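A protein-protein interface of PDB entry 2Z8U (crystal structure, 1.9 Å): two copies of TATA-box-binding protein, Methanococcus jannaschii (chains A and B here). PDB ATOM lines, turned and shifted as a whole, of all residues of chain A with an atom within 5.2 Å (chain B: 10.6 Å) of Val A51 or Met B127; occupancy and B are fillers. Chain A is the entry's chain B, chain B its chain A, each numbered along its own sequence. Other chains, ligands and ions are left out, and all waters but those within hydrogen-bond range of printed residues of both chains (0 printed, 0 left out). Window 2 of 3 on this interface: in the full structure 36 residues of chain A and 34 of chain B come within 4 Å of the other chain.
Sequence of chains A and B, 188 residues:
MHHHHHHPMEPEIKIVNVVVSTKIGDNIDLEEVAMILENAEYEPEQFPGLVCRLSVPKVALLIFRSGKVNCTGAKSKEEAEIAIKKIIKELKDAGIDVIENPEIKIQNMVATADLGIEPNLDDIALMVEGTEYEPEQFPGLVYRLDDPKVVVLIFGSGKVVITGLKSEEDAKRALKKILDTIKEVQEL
No residue of chain B comes within 4 Å of Ala A40. Glu A41 touches none of the printed residues of chain B. Of chain B, only Leu B126 and Met B127 come within 4 Å of Val A51. No residue of chain B comes within 4 Å of Cys A52. Printed residues of chain B within 4 Å of Leu A62: Leu B126 and Met B127. Printed residues of chain A within 4 Å of Leu B126: Val A51 (3.7 Å) and Leu A62 (3.8 Å). Met B127 touches two residues of chain A. Val B128 touches none of the printed residues of chain A. Lys B183 touches none of the printed residues of chain A. Of the printed residues of chain A, Glu B184 touches Phe A47 (3.8 Å). The nearest residue of chain B that does not touch Val A51 is Asp B123 (5.9 Å).
ND2 of Asn B120 sits close to N of Asp B123, 3.0 Å away. O of Asp B180 sits close to OE1 of Glu B184 (2.7 Å). The backbone carbonyl oxygen (O) of Arg A53 lies close to the side-chain amide oxygen (OD1) of Asn A39 (3.2 Å). The backbone NH of Glu A41 sits at hydrogen-bond distance from the backbone carbonyl oxygen of Val A51, 2.7 Å away. The side-chain carboxylate of Glu A41 lies within salt-bridge range of the guanidinium group of Arg A53 (3.2 Å).
Hydrophobic or aromatic side chains of chain A that line the printed part of chain B: Phe A47, Val A51 and Leu A62. Of the 24 printed residues of chain B, 4 touch a printed residue of chain A. Among the printed residues, 6 pairs touch across the chains.
O of Glu B184 touches CD1 of Phe A47, 3.8 Å away. Leu B126 touches Val A51 (CD2 to CG1, 3.7 Å). Met B127 touches Val A51. CD2 of Leu A62 touches O of Leu B126, 3.8 Å away. CA of Met B127 touches CD2 of Leu A62, 3.9 Å away.
OD1 of Asp B123 lies within salt-bridge range of NH1 of Arg A53 (3.2 Å).
No position is printed for both chains.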
ATOM      1  N   ASN A  39      28.621 -33.845 -11.240  1.00  0.00           N
ATOM      2  CA  ASN A  39      28.235 -33.527  -9.861  1.00  0.00           C
ATOM      3  C   ASN A  39      28.155 -32.024  -9.595  1.00  0.00           C
ATOM      4  O   ASN A  39      28.324 -31.592  -8.441  1.00  0.00           O
ATOM      5  CB  ASN A  39      29.218 -34.154  -8.853  1.00  0.00           C
ATOM      6  CG  ASN A  39      29.289 -35.669  -8.951  1.00  0.00           C
ATOM      7  OD1 ASN A  39      30.317 -36.266  -8.633  1.00  0.00           O
ATOM      8  ND2 ASN A  39      28.201 -36.296  -9.384  1.00  0.00           N
ATOM      9  N   ALA A  40      27.930 -31.232 -10.647  1.00  0.00           N
ATOM     10  CA  ALA A  40      27.940 -29.766 -10.534  1.00  0.00           C
ATOM     11  C   ALA A  40      26.535 -29.252 -10.329  1.00  0.00           C
ATOM     12  O   ALA A  40      25.604 -29.648 -11.049  1.00  0.00           O
ATOM     13  CB  ALA A  40      28.562 -29.115 -11.775  1.00  0.00           C
ATOM     14  N   GLU A  41      26.378 -28.393  -9.333  1.00  0.00           N
ATOM     15  CA  GLU A  41      25.114 -27.708  -9.070  1.00  0.00           C
ATOM     16  C   GLU A  41      25.304 -26.228  -9.390  1.00  0.00           C
ATOM     17  O   GLU A  41      26.158 -25.558  -8.776  1.00  0.00           O
ATOM     18  CB  GLU A  41      24.726 -27.897  -7.605  1.00  0.00           C
ATOM     19  CG  GLU A  41      23.362 -27.320  -7.226  1.00  0.00           C
ATOM     20  CD  GLU A  41      23.033 -27.437  -5.731  1.00  0.00           C
ATOM     21  OE1 GLU A  41      23.872 -27.941  -4.953  1.00  0.00           O
ATOM     22  OE2 GLU A  41      21.919 -27.018  -5.334  1.00  0.00           O
ATOM     23  N   TYR A  42      24.540 -25.723 -10.357  1.00  0.00           N
ATOM     24  CA  TYR A  42      24.623 -24.313 -10.749  1.00  0.00           C
ATOM     25  C   TYR A  42      23.251 -23.726 -11.071  1.00  0.00           C
ATOM     26  O   TYR A  42      22.629 -24.104 -12.059  1.00  0.00           O
ATOM     27  CB  TYR A  42      25.580 -24.135 -11.943  1.00  0.00           C
ATOM     28  CG  TYR A  42      25.760 -22.706 -12.415  1.00  0.00           C
ATOM     29  CD1 TYR A  42      26.138 -21.693 -11.527  1.00  0.00           C
ATOM     30  CD2 TYR A  42      25.575 -22.371 -13.753  1.00  0.00           C
ATOM     31  CE1 TYR A  42      26.309 -20.383 -11.962  1.00  0.00           C
ATOM     32  CE2 TYR A  42      25.749 -21.069 -14.197  1.00  0.00           C
ATOM     33  CZ  TYR A  42      26.123 -20.080 -13.293  1.00  0.00           C
ATOM     34  OH  TYR A  42      26.289 -18.777 -13.731  1.00  0.00           O
ATOM     35  N   PHE A  47      21.650 -18.368  -6.877  1.00  0.00           N
ATOM     36  CA  PHE A  47      22.944 -18.219  -6.222  1.00  0.00           C
ATOM     37  C   PHE A  47      24.049 -18.093  -7.299  1.00  0.00           C
ATOM     38  O   PHE A  47      24.025 -18.820  -8.295  1.00  0.00           O
ATOM     39  CB  PHE A  47      23.199 -19.424  -5.297  1.00  0.00           C
ATOM     40  CG  PHE A  47      24.498 -19.359  -4.560  1.00  0.00           C
ATOM     41  CD1 PHE A  47      24.636 -18.558  -3.432  1.00  0.00           C
ATOM     42  CD2 PHE A  47      25.596 -20.092  -4.997  1.00  0.00           C
ATOM     43  CE1 PHE A  47      25.851 -18.489  -2.748  1.00  0.00           C
ATOM     44  CE2 PHE A  47      26.817 -20.028  -4.324  1.00  0.00           C
ATOM     45  CZ  PHE A  47      26.946 -19.228  -3.196  1.00  0.00           C
ATOM     46  N   GLY A  49      27.326 -18.728  -7.414  1.00  0.00           N
ATOM     47  CA  GLY A  49      28.464 -19.671  -7.462  1.00  0.00           C
ATOM     48  C   GLY A  49      28.090 -21.066  -7.940  1.00  0.00           C
ATOM     49  O   GLY A  49      26.912 -21.463  -7.903  1.00  0.00           O
ATOM     50  N   LEU A  50      29.088 -21.813  -8.408  1.00  0.00           N
ATOM     51  CA  LEU A  50      28.872 -23.190  -8.851  1.00  0.00           C
ATOM     52  C   LEU A  50      29.448 -24.143  -7.826  1.00  0.00           C
ATOM     53  O   LEU A  50      30.578 -23.946  -7.365  1.00  0.00           O
ATOM     54  CB  LEU A  50      29.517 -23.439 -10.232  1.00  0.00           C
ATOM     55  CG  LEU A  50      29.473 -24.855 -10.804  1.00  0.00           C
ATOM     56  CD1 LEU A  50      29.400 -24.793 -12.316  1.00  0.00           C
ATOM     57  CD2 LEU A  50      30.640 -25.736 -10.339  1.00  0.00           C
ATOM     58  N   VAL A  51      28.703 -25.202  -7.514  1.00  0.00           N
ATOM     59  CA  VAL A  51      29.138 -26.206  -6.529  1.00  0.00           C
ATOM     60  C   VAL A  51      29.476 -27.524  -7.208  1.00  0.00           C
ATOM     61  O   VAL A  51      28.684 -28.032  -7.988  1.00  0.00           O
ATOM     62  CB  VAL A  51      28.060 -26.452  -5.432  1.00  0.00           C
ATOM     63  CG1 VAL A  51      28.522 -27.507  -4.428  1.00  0.00           C
ATOM     64  CG2 VAL A  51      27.713 -25.148  -4.725  1.00  0.00           C
ATOM     65  N   CYS A  52      30.671 -28.048  -6.931  1.00  0.00           N
ATOM     66  CA  CYS A  52      31.093 -29.353  -7.424  1.00  0.00           C
ATOM     67  C   CYS A  52      31.477 -30.241  -6.240  1.00  0.00           C
ATOM     68  O   CYS A  52      32.356 -29.894  -5.454  1.00  0.00           O
ATOM     69  CB  CYS A  52      32.274 -29.248  -8.389  1.00  0.00           C
ATOM     70  SG  CYS A  52      32.807 -30.918  -9.018  1.00  0.00           S
ATOM     71  N   ARG A  53      30.810 -31.382  -6.120  1.00  0.00           N
ATOM     72  CA  ARG A  53      31.045 -32.300  -5.008  1.00  0.00           C
ATOM     73  C   ARG A  53      31.726 -33.563  -5.492  1.00  0.00           C
ATOM     74  O   ARG A  53      31.119 -34.378  -6.189  1.00  0.00           O
ATOM     75  CB  ARG A  53      29.743 -32.625  -4.285  1.00  0.00           C
ATOM     76  CG  ARG A  53      29.402 -31.640  -3.185  1.00  0.00           C
ATOM     77  CD  ARG A  53      28.100 -32.011  -2.506  1.00  0.00           C
ATOM     78  NE  ARG A  53      27.011 -31.135  -2.930  1.00  0.00           N
ATOM     79  CZ  ARG A  53      26.584 -30.091  -2.225  1.00  0.00           C
ATOM     80  NH1 ARG A  53      27.154 -29.803  -1.052  1.00  0.00           N
ATOM     81  NH2 ARG A  53      25.585 -29.338  -2.687  1.00  0.00           N
ATOM     82  N   LEU A  61      33.862 -28.168  -3.911  1.00  0.00           N
ATOM     83  CA  LEU A  61      34.412 -26.895  -4.369  1.00  0.00           C
ATOM     84  C   LEU A  61      33.269 -25.950  -4.696  1.00  0.00           C
ATOM     85  O   LEU A  61      32.239 -26.373  -5.228  1.00  0.00           O
ATOM     86  CB  LEU A  61      35.298 -27.099  -5.612  1.00  0.00           C
ATOM     87  CG  LEU A  61      36.589 -27.936  -5.478  1.00  0.00           C
ATOM     88  CD1 LEU A  61      36.336 -29.412  -5.773  1.00  0.00           C
ATOM     89  CD2 LEU A  61      37.603 -27.419  -6.454  1.00  0.00           C
ATOM     90  N   LEU A  62      33.464 -24.676  -4.372  1.00  0.00           N
ATOM     91  CA  LEU A  62      32.562 -23.613  -4.742  1.00  0.00           C
ATOM     92  C   LEU A  62      33.350 -22.706  -5.665  1.00  0.00           C
ATOM     93  O   LEU A  62      34.433 -22.229  -5.299  1.00  0.00           O
ATOM     94  CB  LEU A  62      32.067 -22.853  -3.504  1.00  0.00           C
ATOM     95  CG  LEU A  62      31.239 -21.564  -3.682  1.00  0.00           C
ATOM     96  CD1 LEU A  62      29.960 -21.775  -4.470  1.00  0.00           C
ATOM     97  CD2 LEU A  62      30.927 -20.952  -2.315  1.00  0.00           C
ATOM     98  N   ILE A  63      32.845 -22.543  -6.890  1.00  0.00           N
ATOM     99  CA  ILE A  63      33.555 -21.775  -7.902  1.00  0.00           C
ATOM    100  C   ILE A  63      32.756 -20.536  -8.318  1.00  0.00           C
ATOM    101  O   ILE A  63      31.590 -20.655  -8.693  1.00  0.00           O
ATOM    102  CB  ILE A  63      33.843 -22.616  -9.172  1.00  0.00           C
ATOM    103  CG1 ILE A  63      34.487 -23.966  -8.806  1.00  0.00           C
ATOM    104  CG2 ILE A  63      34.696 -21.795 -10.163  1.00  0.00           C
ATOM    105  CD1 ILE A  63      34.723 -24.896  -9.978  1.00  0.00           C
ATOM    106  N   PRO B 119      18.370 -26.549   8.277  1.00  0.00           N
ATOM    107  CA  PRO B 119      19.416 -26.185   7.320  1.00  0.00           C
ATOM    108  C   PRO B 119      20.259 -27.372   6.806  1.00  0.00           C
ATOM    109  O   PRO B 119      20.314 -28.437   7.435  1.00  0.00           O
ATOM    110  CB  PRO B 119      20.283 -25.215   8.129  1.00  0.00           C
ATOM    111  CG  PRO B 119      20.174 -25.708   9.511  1.00  0.00           C
ATOM    112  CD  PRO B 119      18.793 -26.291   9.665  1.00  0.00           C
ATOM    113  N   ASN B 120      20.895 -27.175   5.654  1.00  0.00           N
ATOM    114  CA  ASN B 120      21.859 -28.128   5.120  1.00  0.00           C
ATOM    115  C   ASN B 120      23.227 -27.671   5.582  1.00  0.00           C
ATOM    116  O   ASN B 120      23.785 -26.691   5.078  1.00  0.00           O
ATOM    117  CB  ASN B 120      21.797 -28.186   3.592  1.00  0.00           C
ATOM    118  CG  ASN B 120      22.557 -29.372   3.010  1.00  0.00           C
ATOM    119  OD1 ASN B 120      22.009 -30.131   2.216  1.00  0.00           O
ATOM    120  ND2 ASN B 120      23.819 -29.523   3.376  1.00  0.00           N
ATOM    121  N   LEU B 121      23.755 -28.377   6.576  1.00  0.00           N
ATOM    122  CA  LEU B 121      24.974 -27.935   7.235  1.00  0.00           C
ATOM    123  C   LEU B 121      26.186 -28.059   6.305  1.00  0.00           C
ATOM    124  O   LEU B 121      27.085 -27.234   6.357  1.00  0.00           O
ATOM    125  CB  LEU B 121      25.158 -28.654   8.585  1.00  0.00           C
ATOM    126  CG  LEU B 121      24.033 -28.489   9.629  1.00  0.00           C
ATOM    127  CD1 LEU B 121      24.380 -29.215  10.927  1.00  0.00           C
ATOM    128  CD2 LEU B 121      23.654 -27.030   9.929  1.00  0.00           C
ATOM    129  N   ASP B 122      26.184 -29.054   5.417  1.00  0.00           N
ATOM    130  CA  ASP B 122      27.256 -29.166   4.416  1.00  0.00           C
ATOM    131  C   ASP B 122      27.249 -27.979   3.458  1.00  0.00           C
ATOM    132  O   ASP B 122      28.309 -27.441   3.128  1.00  0.00           O
ATOM    133  CB  ASP B 122      27.159 -30.472   3.626  1.00  0.00           C
ATOM    134  CG  ASP B 122      27.506 -31.687   4.466  1.00  0.00           C
ATOM    135  OD1 ASP B 122      26.634 -32.572   4.599  1.00  0.00           O
ATOM    136  OD2 ASP B 122      28.639 -31.751   4.999  1.00  0.00           O
ATOM    137  N   ASP B 123      26.053 -27.581   3.026  1.00  0.00           N
ATOM    138  CA  ASP B 123      25.885 -26.402   2.179  1.00  0.00           C
ATOM    139  C   ASP B 123      26.423 -25.136   2.852  1.00  0.00           C
ATOM    140  O   ASP B 123      27.197 -24.398   2.238  1.00  0.00           O
ATOM    141  CB  ASP B 123      24.418 -26.220   1.768  1.00  0.00           C
ATOM    142  CG  ASP B 123      23.998 -27.180   0.678  1.00  0.00           C
ATOM    143  OD1 ASP B 123      24.862 -27.913   0.147  1.00  0.00           O
ATOM    144  OD2 ASP B 123      22.801 -27.198   0.348  1.00  0.00           O
ATOM    145  N   ILE B 124      26.016 -24.886   4.101  1.00  0.00           N
ATOM    146  CA  ILE B 124      26.535 -23.731   4.854  1.00  0.00           C
ATOM    147  C   ILE B 124      28.060 -23.762   5.012  1.00  0.00           C
ATOM    148  O   ILE B 124      28.732 -22.749   4.805  1.00  0.00           O
ATOM    149  CB  ILE B 124      25.882 -23.586   6.262  1.00  0.00           C
ATOM    150  CG1 ILE B 124      24.357 -23.454   6.134  1.00  0.00           C
ATOM    151  CG2 ILE B 124      26.495 -22.388   7.025  1.00  0.00           C
ATOM    152  CD1 ILE B 124      23.587 -23.627   7.454  1.00  0.00           C
ATOM    153  N   ALA B 125      28.600 -24.918   5.380  1.00  0.00           N
ATOM    154  CA  ALA B 125      30.028 -25.022   5.660  1.00  0.00           C
ATOM    155  C   ALA B 125      30.884 -24.704   4.427  1.00  0.00           C
ATOM    156  O   ALA B 125      32.007 -24.209   4.553  1.00  0.00           O
ATOM    157  CB  ALA B 125      30.343 -26.393   6.183  1.00  0.00           C
ATOM    158  N   LEU B 126      30.357 -25.010   3.239  1.00  0.00           N
ATOM    159  CA  LEU B 126      31.032 -24.652   1.990  1.00  0.00           C
ATOM    160  C   LEU B 126      30.792 -23.205   1.550  1.00  0.00           C
ATOM    161  O   LEU B 126      31.698 -22.548   0.998  1.00  0.00           O
ATOM    162  CB  LEU B 126      30.609 -25.615   0.865  1.00  0.00           C
ATOM    163  CG  LEU B 126      31.179 -25.334  -0.526  1.00  0.00           C
ATOM    164  CD1 LEU B 126      32.726 -25.518  -0.571  1.00  0.00           C
ATOM    165  CD2 LEU B 126      30.435 -26.148  -1.601  1.00  0.00           C
ATOM    166  N   MET B 127      29.567 -22.722   1.767  1.00  0.00           N
ATOM    167  CA  MET B 127      29.107 -21.489   1.115  1.00  0.00           C
ATOM    168  C   MET B 127      29.207 -20.259   2.013  1.00  0.00           C
ATOM    169  O   MET B 127      29.089 -19.133   1.528  1.00  0.00           O
ATOM    170  CB  MET B 127      27.677 -21.656   0.572  1.00  0.00           C
ATOM    171  CG  MET B 127      27.514 -22.795  -0.418  1.00  0.00           C
ATOM    172  SD  MET B 127      25.808 -23.003  -0.975  1.00  0.00           S
ATOM    173  CE  MET B 127      25.973 -24.311  -2.174  1.00  0.00           C
ATOM    174  N   VAL B 128      29.430 -20.488   3.308  1.00  0.00           N
ATOM    175  CA  VAL B 128      29.622 -19.417   4.287  1.00  0.00           C
ATOM    176  C   VAL B 128      31.000 -19.475   4.947  1.00  0.00           C
ATOM    177  O   VAL B 128      31.417 -20.511   5.492  1.00  0.00           O
ATOM    178  CB  VAL B 128      28.528 -19.430   5.384  1.00  0.00           C
ATOM    179  CG1 VAL B 128      28.732 -18.269   6.390  1.00  0.00           C
ATOM    180  CG2 VAL B 128      27.142 -19.377   4.755  1.00  0.00           C
ATOM    181  N   GLU B 129      31.696 -18.343   4.911  1.00  0.00           N
ATOM    182  CA  GLU B 129      33.032 -18.250   5.481  1.00  0.00           C
ATOM    183  C   GLU B 129      32.997 -18.134   7.013  1.00  0.00           C
ATOM    184  O   GLU B 129      32.014 -17.672   7.592  1.00  0.00           O
ATOM    185  CB  GLU B 129      33.825 -17.130   4.779  1.00  0.00           C
ATOM    186  CG  GLU B 129      34.046 -17.436   3.276  1.00  0.00           C
ATOM    187  CD  GLU B 129      34.618 -16.277   2.445  1.00  0.00           C
ATOM    188  OE1 GLU B 129      34.502 -15.095   2.839  1.00  0.00           O
ATOM    189  OE2 GLU B 129      35.172 -16.556   1.367  1.00  0.00           O
ATOM    190  N   GLY B 130      34.049 -18.613   7.676  1.00  0.00           N
ATOM    191  CA  GLY B 130      34.082 -18.638   9.153  1.00  0.00           C
ATOM    192  C   GLY B 130      33.161 -19.658   9.789  1.00  0.00           C
ATOM    193  O   GLY B 130      32.706 -19.488  10.940  1.00  0.00           O
ATOM    194  N   THR B 131      32.851 -20.704   9.026  1.00  0.00           N
ATOM    195  CA  THR B 131      32.107 -21.842   9.552  1.00  0.00           C
ATOM    196  C   THR B 131      32.994 -23.064   9.500  1.00  0.00           C
ATOM    197  O   THR B 131      33.905 -23.136   8.675  1.00  0.00           O
ATOM    198  CB  THR B 131      30.845 -22.146   8.723  1.00  0.00           C
ATOM    199  OG1 THR B 131      31.231 -22.455   7.383  1.00  0.00           O
ATOM    200  CG2 THR B 131      29.896 -20.960   8.712  1.00  0.00           C
ATOM    201  N   GLU B 132      32.743 -24.000  10.410  1.00  0.00           N
ATOM    202  CA  GLU B 132      33.326 -25.322  10.368  1.00  0.00           C
ATOM    203  C   GLU B 132      32.250 -26.340  10.709  1.00  0.00           C
ATOM    204  O   GLU B 132      31.275 -26.048  11.418  1.00  0.00           O
ATOM    205  CB  GLU B 132      34.551 -25.455  11.300  1.00  0.00           C
ATOM    206  CG  GLU B 132      35.919 -25.351  10.573  1.00  0.00           C
ATOM    207  CD  GLU B 132      36.221 -26.491   9.588  1.00  0.00           C
ATOM    208  OE1 GLU B 132      35.317 -27.317   9.265  1.00  0.00           O
ATOM    209  OE2 GLU B 132      37.397 -26.574   9.143  1.00  0.00           O
ATOM    210  N   TYR B 133      32.439 -27.544  10.185  1.00  0.00           N
ATOM    211  CA  TYR B 133      31.490 -28.612  10.359  1.00  0.00           C
ATOM    212  C   TYR B 133      32.281 -29.909  10.246  1.00  0.00           C
ATOM    213  O   TYR B 133      33.110 -30.071   9.346  1.00  0.00           O
ATOM    214  CB  TYR B 133      30.396 -28.488   9.297  1.00  0.00           C
ATOM    215  CG  TYR B 133      29.315 -29.539   9.348  1.00  0.00           C
ATOM    216  CD1 TYR B 133      28.683 -29.869  10.552  1.00  0.00           C
ATOM    217  CD2 TYR B 133      28.912 -30.201   8.182  1.00  0.00           C
ATOM    218  CE1 TYR B 133      27.688 -30.849  10.599  1.00  0.00           C
ATOM    219  CE2 TYR B 133      27.911 -31.165   8.217  1.00  0.00           C
ATOM    220  CZ  TYR B 133      27.304 -31.482   9.427  1.00  0.00           C
ATOM    221  OH  TYR B 133      26.316 -32.450   9.462  1.00  0.00           O
ATOM    222  N   LEU B 141      27.103 -27.205  13.388  1.00  0.00           N
ATOM    223  CA  LEU B 141      28.019 -26.374  12.663  1.00  0.00           C
ATOM    224  C   LEU B 141      28.426 -25.216  13.568  1.00  0.00           C
ATOM    225  O   LEU B 141      27.575 -24.637  14.248  1.00  0.00           O
ATOM    226  CB  LEU B 141      27.320 -25.851  11.405  1.00  0.00           C
ATOM    227  CG  LEU B 141      28.115 -24.871  10.541  1.00  0.00           C
ATOM    228  CD1 LEU B 141      27.934 -25.206   9.058  1.00  0.00           C
ATOM    229  CD2 LEU B 141      27.714 -23.421  10.824  1.00  0.00           C
ATOM    230  N   TYR B 143      29.775 -21.441  13.890  1.00  0.00           N
ATOM    231  CA  TYR B 143      29.842 -20.180  13.162  1.00  0.00           C
ATOM    232  C   TYR B 143      30.306 -19.028  14.070  1.00  0.00           C
ATOM    233  O   TYR B 143      29.627 -18.652  15.032  1.00  0.00           O
ATOM    234  CB  TYR B 143      28.491 -19.851  12.547  1.00  0.00           C
ATOM    235  CG  TYR B 143      28.488 -18.651  11.608  1.00  0.00           C
ATOM    236  CD1 TYR B 143      29.625 -18.288  10.871  1.00  0.00           C
ATOM    237  CD2 TYR B 143      27.333 -17.919  11.415  1.00  0.00           C
ATOM    238  CE1 TYR B 143      29.595 -17.184   9.981  1.00  0.00           C
ATOM    239  CE2 TYR B 143      27.292 -16.824  10.522  1.00  0.00           C
ATOM    240  CZ  TYR B 143      28.418 -16.460   9.828  1.00  0.00           C
ATOM    241  OH  TYR B 143      28.353 -15.383   8.946  1.00  0.00           O
ATOM    242  N   ASP B 180      19.996 -14.077   7.843  1.00  0.00           N
ATOM    243  CA  ASP B 180      20.277 -13.448   6.562  1.00  0.00           C
ATOM    244  C   ASP B 180      21.306 -14.236   5.755  1.00  0.00           C
ATOM    245  O   ASP B 180      21.127 -14.423   4.551  1.00  0.00           O
ATOM    246  CB  ASP B 180      20.724 -11.992   6.754  1.00  0.00           C
ATOM    247  CG  ASP B 180      19.566 -11.065   7.130  1.00  0.00           C
ATOM    248  OD1 ASP B 180      18.400 -11.530   7.162  1.00  0.00           O
ATOM    249  OD2 ASP B 180      19.829  -9.869   7.390  1.00  0.00           O
ATOM    250  N   THR B 181      22.358 -14.714   6.417  1.00  0.00           N
ATOM    251  CA  THR B 181      23.393 -15.506   5.736  1.00  0.00           C
ATOM    252  C   THR B 181      22.848 -16.864   5.292  1.00  0.00           C
ATOM    253  O   THR B 181      23.126 -17.315   4.187  1.00  0.00           O
ATOM    254  CB  THR B 181      24.665 -15.700   6.598  1.00  0.00           C
ATOM    255  OG1 THR B 181      24.868 -14.552   7.432  1.00  0.00           O
ATOM    256  CG2 THR B 181      25.891 -15.890   5.697  1.00  0.00           C
ATOM    257  N   ILE B 182      22.050 -17.493   6.146  1.00  0.00           N
ATOM    258  CA  ILE B 182      21.438 -18.786   5.832  1.00  0.00           C
ATOM    259  C   ILE B 182      20.313 -18.694   4.774  1.00  0.00           C
ATOM    260  O   ILE B 182      20.085 -19.650   4.024  1.00  0.00           O
ATOM    261  CB  ILE B 182      20.971 -19.506   7.125  1.00  0.00           C
ATOM    262  CG1 ILE B 182      22.178 -19.767   8.034  1.00  0.00           C
ATOM    263  CG2 ILE B 182      20.251 -20.826   6.812  1.00  0.00           C
ATOM    264  CD1 ILE B 182      21.816 -20.374   9.362  1.00  0.00           C
ATOM    265  N   LYS B 183      19.627 -17.551   4.706  1.00  0.00           N
ATOM    266  CA  LYS B 183      18.650 -17.301   3.634  1.00  0.00           C
ATOM    267  C   LYS B 183      19.360 -17.292   2.285  1.00  0.00           C
ATOM    268  O   LYS B 183      18.823 -17.768   1.286  1.00  0.00           O
ATOM    269  CB  LYS B 183      17.919 -15.966   3.827  1.00  0.00           C
ATOM    270  CG  LYS B 183      16.936 -15.910   4.996  1.00  0.00           C
ATOM    271  CD  LYS B 183      16.245 -14.539   5.064  1.00  0.00           C
ATOM    272  CE  LYS B 183      15.943 -14.114   6.505  1.00  0.00           C
ATOM    273  NZ  LYS B 183      14.818 -14.870   7.129  1.00  0.00           N
ATOM    274  N   GLU B 184      20.575 -16.746   2.276  1.00  0.00           N
ATOM    275  CA  GLU B 184      21.425 -16.700   1.084  1.00  0.00           C
ATOM    276  C   GLU B 184      21.916 -18.089   0.653  1.00  0.00           C
ATOM    277  O   GLU B 184      22.254 -18.301  -0.511  1.00  0.00           O
ATOM    278  CB  GLU B 184      22.623 -15.776   1.325  1.00  0.00           C
ATOM    279  CG  GLU B 184      22.254 -14.318   1.611  1.00  0.00           C
ATOM    280  CD  GLU B 184      23.292 -13.605   2.473  1.00  0.00           C
ATOM    281  OE1 GLU B 184      22.891 -12.791   3.335  1.00  0.00           O
ATOM    282  OE2 GLU B 184      24.506 -13.863   2.306  1.00  0.00           O
ATOM    283  N   VAL B 185      21.959 -19.024   1.600  1.00  0.00           N
ATOM    284  CA  VAL B 185      22.393 -20.394   1.321  1.00  0.00           C
ATOM    285  C   VAL B 185      21.238 -21.262   0.812  1.00  0.00           C
ATOM    286  O   VAL B 185      21.410 -22.026  -0.137  1.00  0.00           O
ATOM    287  CB  VAL B 185      23.130 -21.025   2.547  1.00  0.00           C
ATOM    288  CG1 VAL B 185      22.993 -22.546   2.591  1.00  0.00           C
ATOM    289  CG2 VAL B 185      24.594 -20.630   2.526  1.00  0.00           C
ATOM    290  N   GLN B 186      20.065 -21.134   1.431  1.00  0.00           N
ATOM    291  CA  GLN B 186      18.893 -21.906   1.011  1.00  0.00           C
ATOM    292  C   GLN B 186      17.760 -21.029   0.502  1.00  0.00           C
ATOM    293  O   GLN B 186      17.487 -20.997  -0.699  1.00  0.00           O
ATOM    294  CB  GLN B 186      18.412 -22.819   2.139  1.00  0.00           C
ATOM    295  CG  GLN B 186      19.264 -24.079   2.275  1.00  0.00           C
ATOM    296  CD  GLN B 186      19.383 -24.572   3.706  1.00  0.00           C
ATOM    297  OE1 GLN B 186      18.399 -24.991   4.317  1.00  0.00           O
ATOM    298  NE2 GLN B 186      20.598 -24.535   4.243  1.00  0.00           N
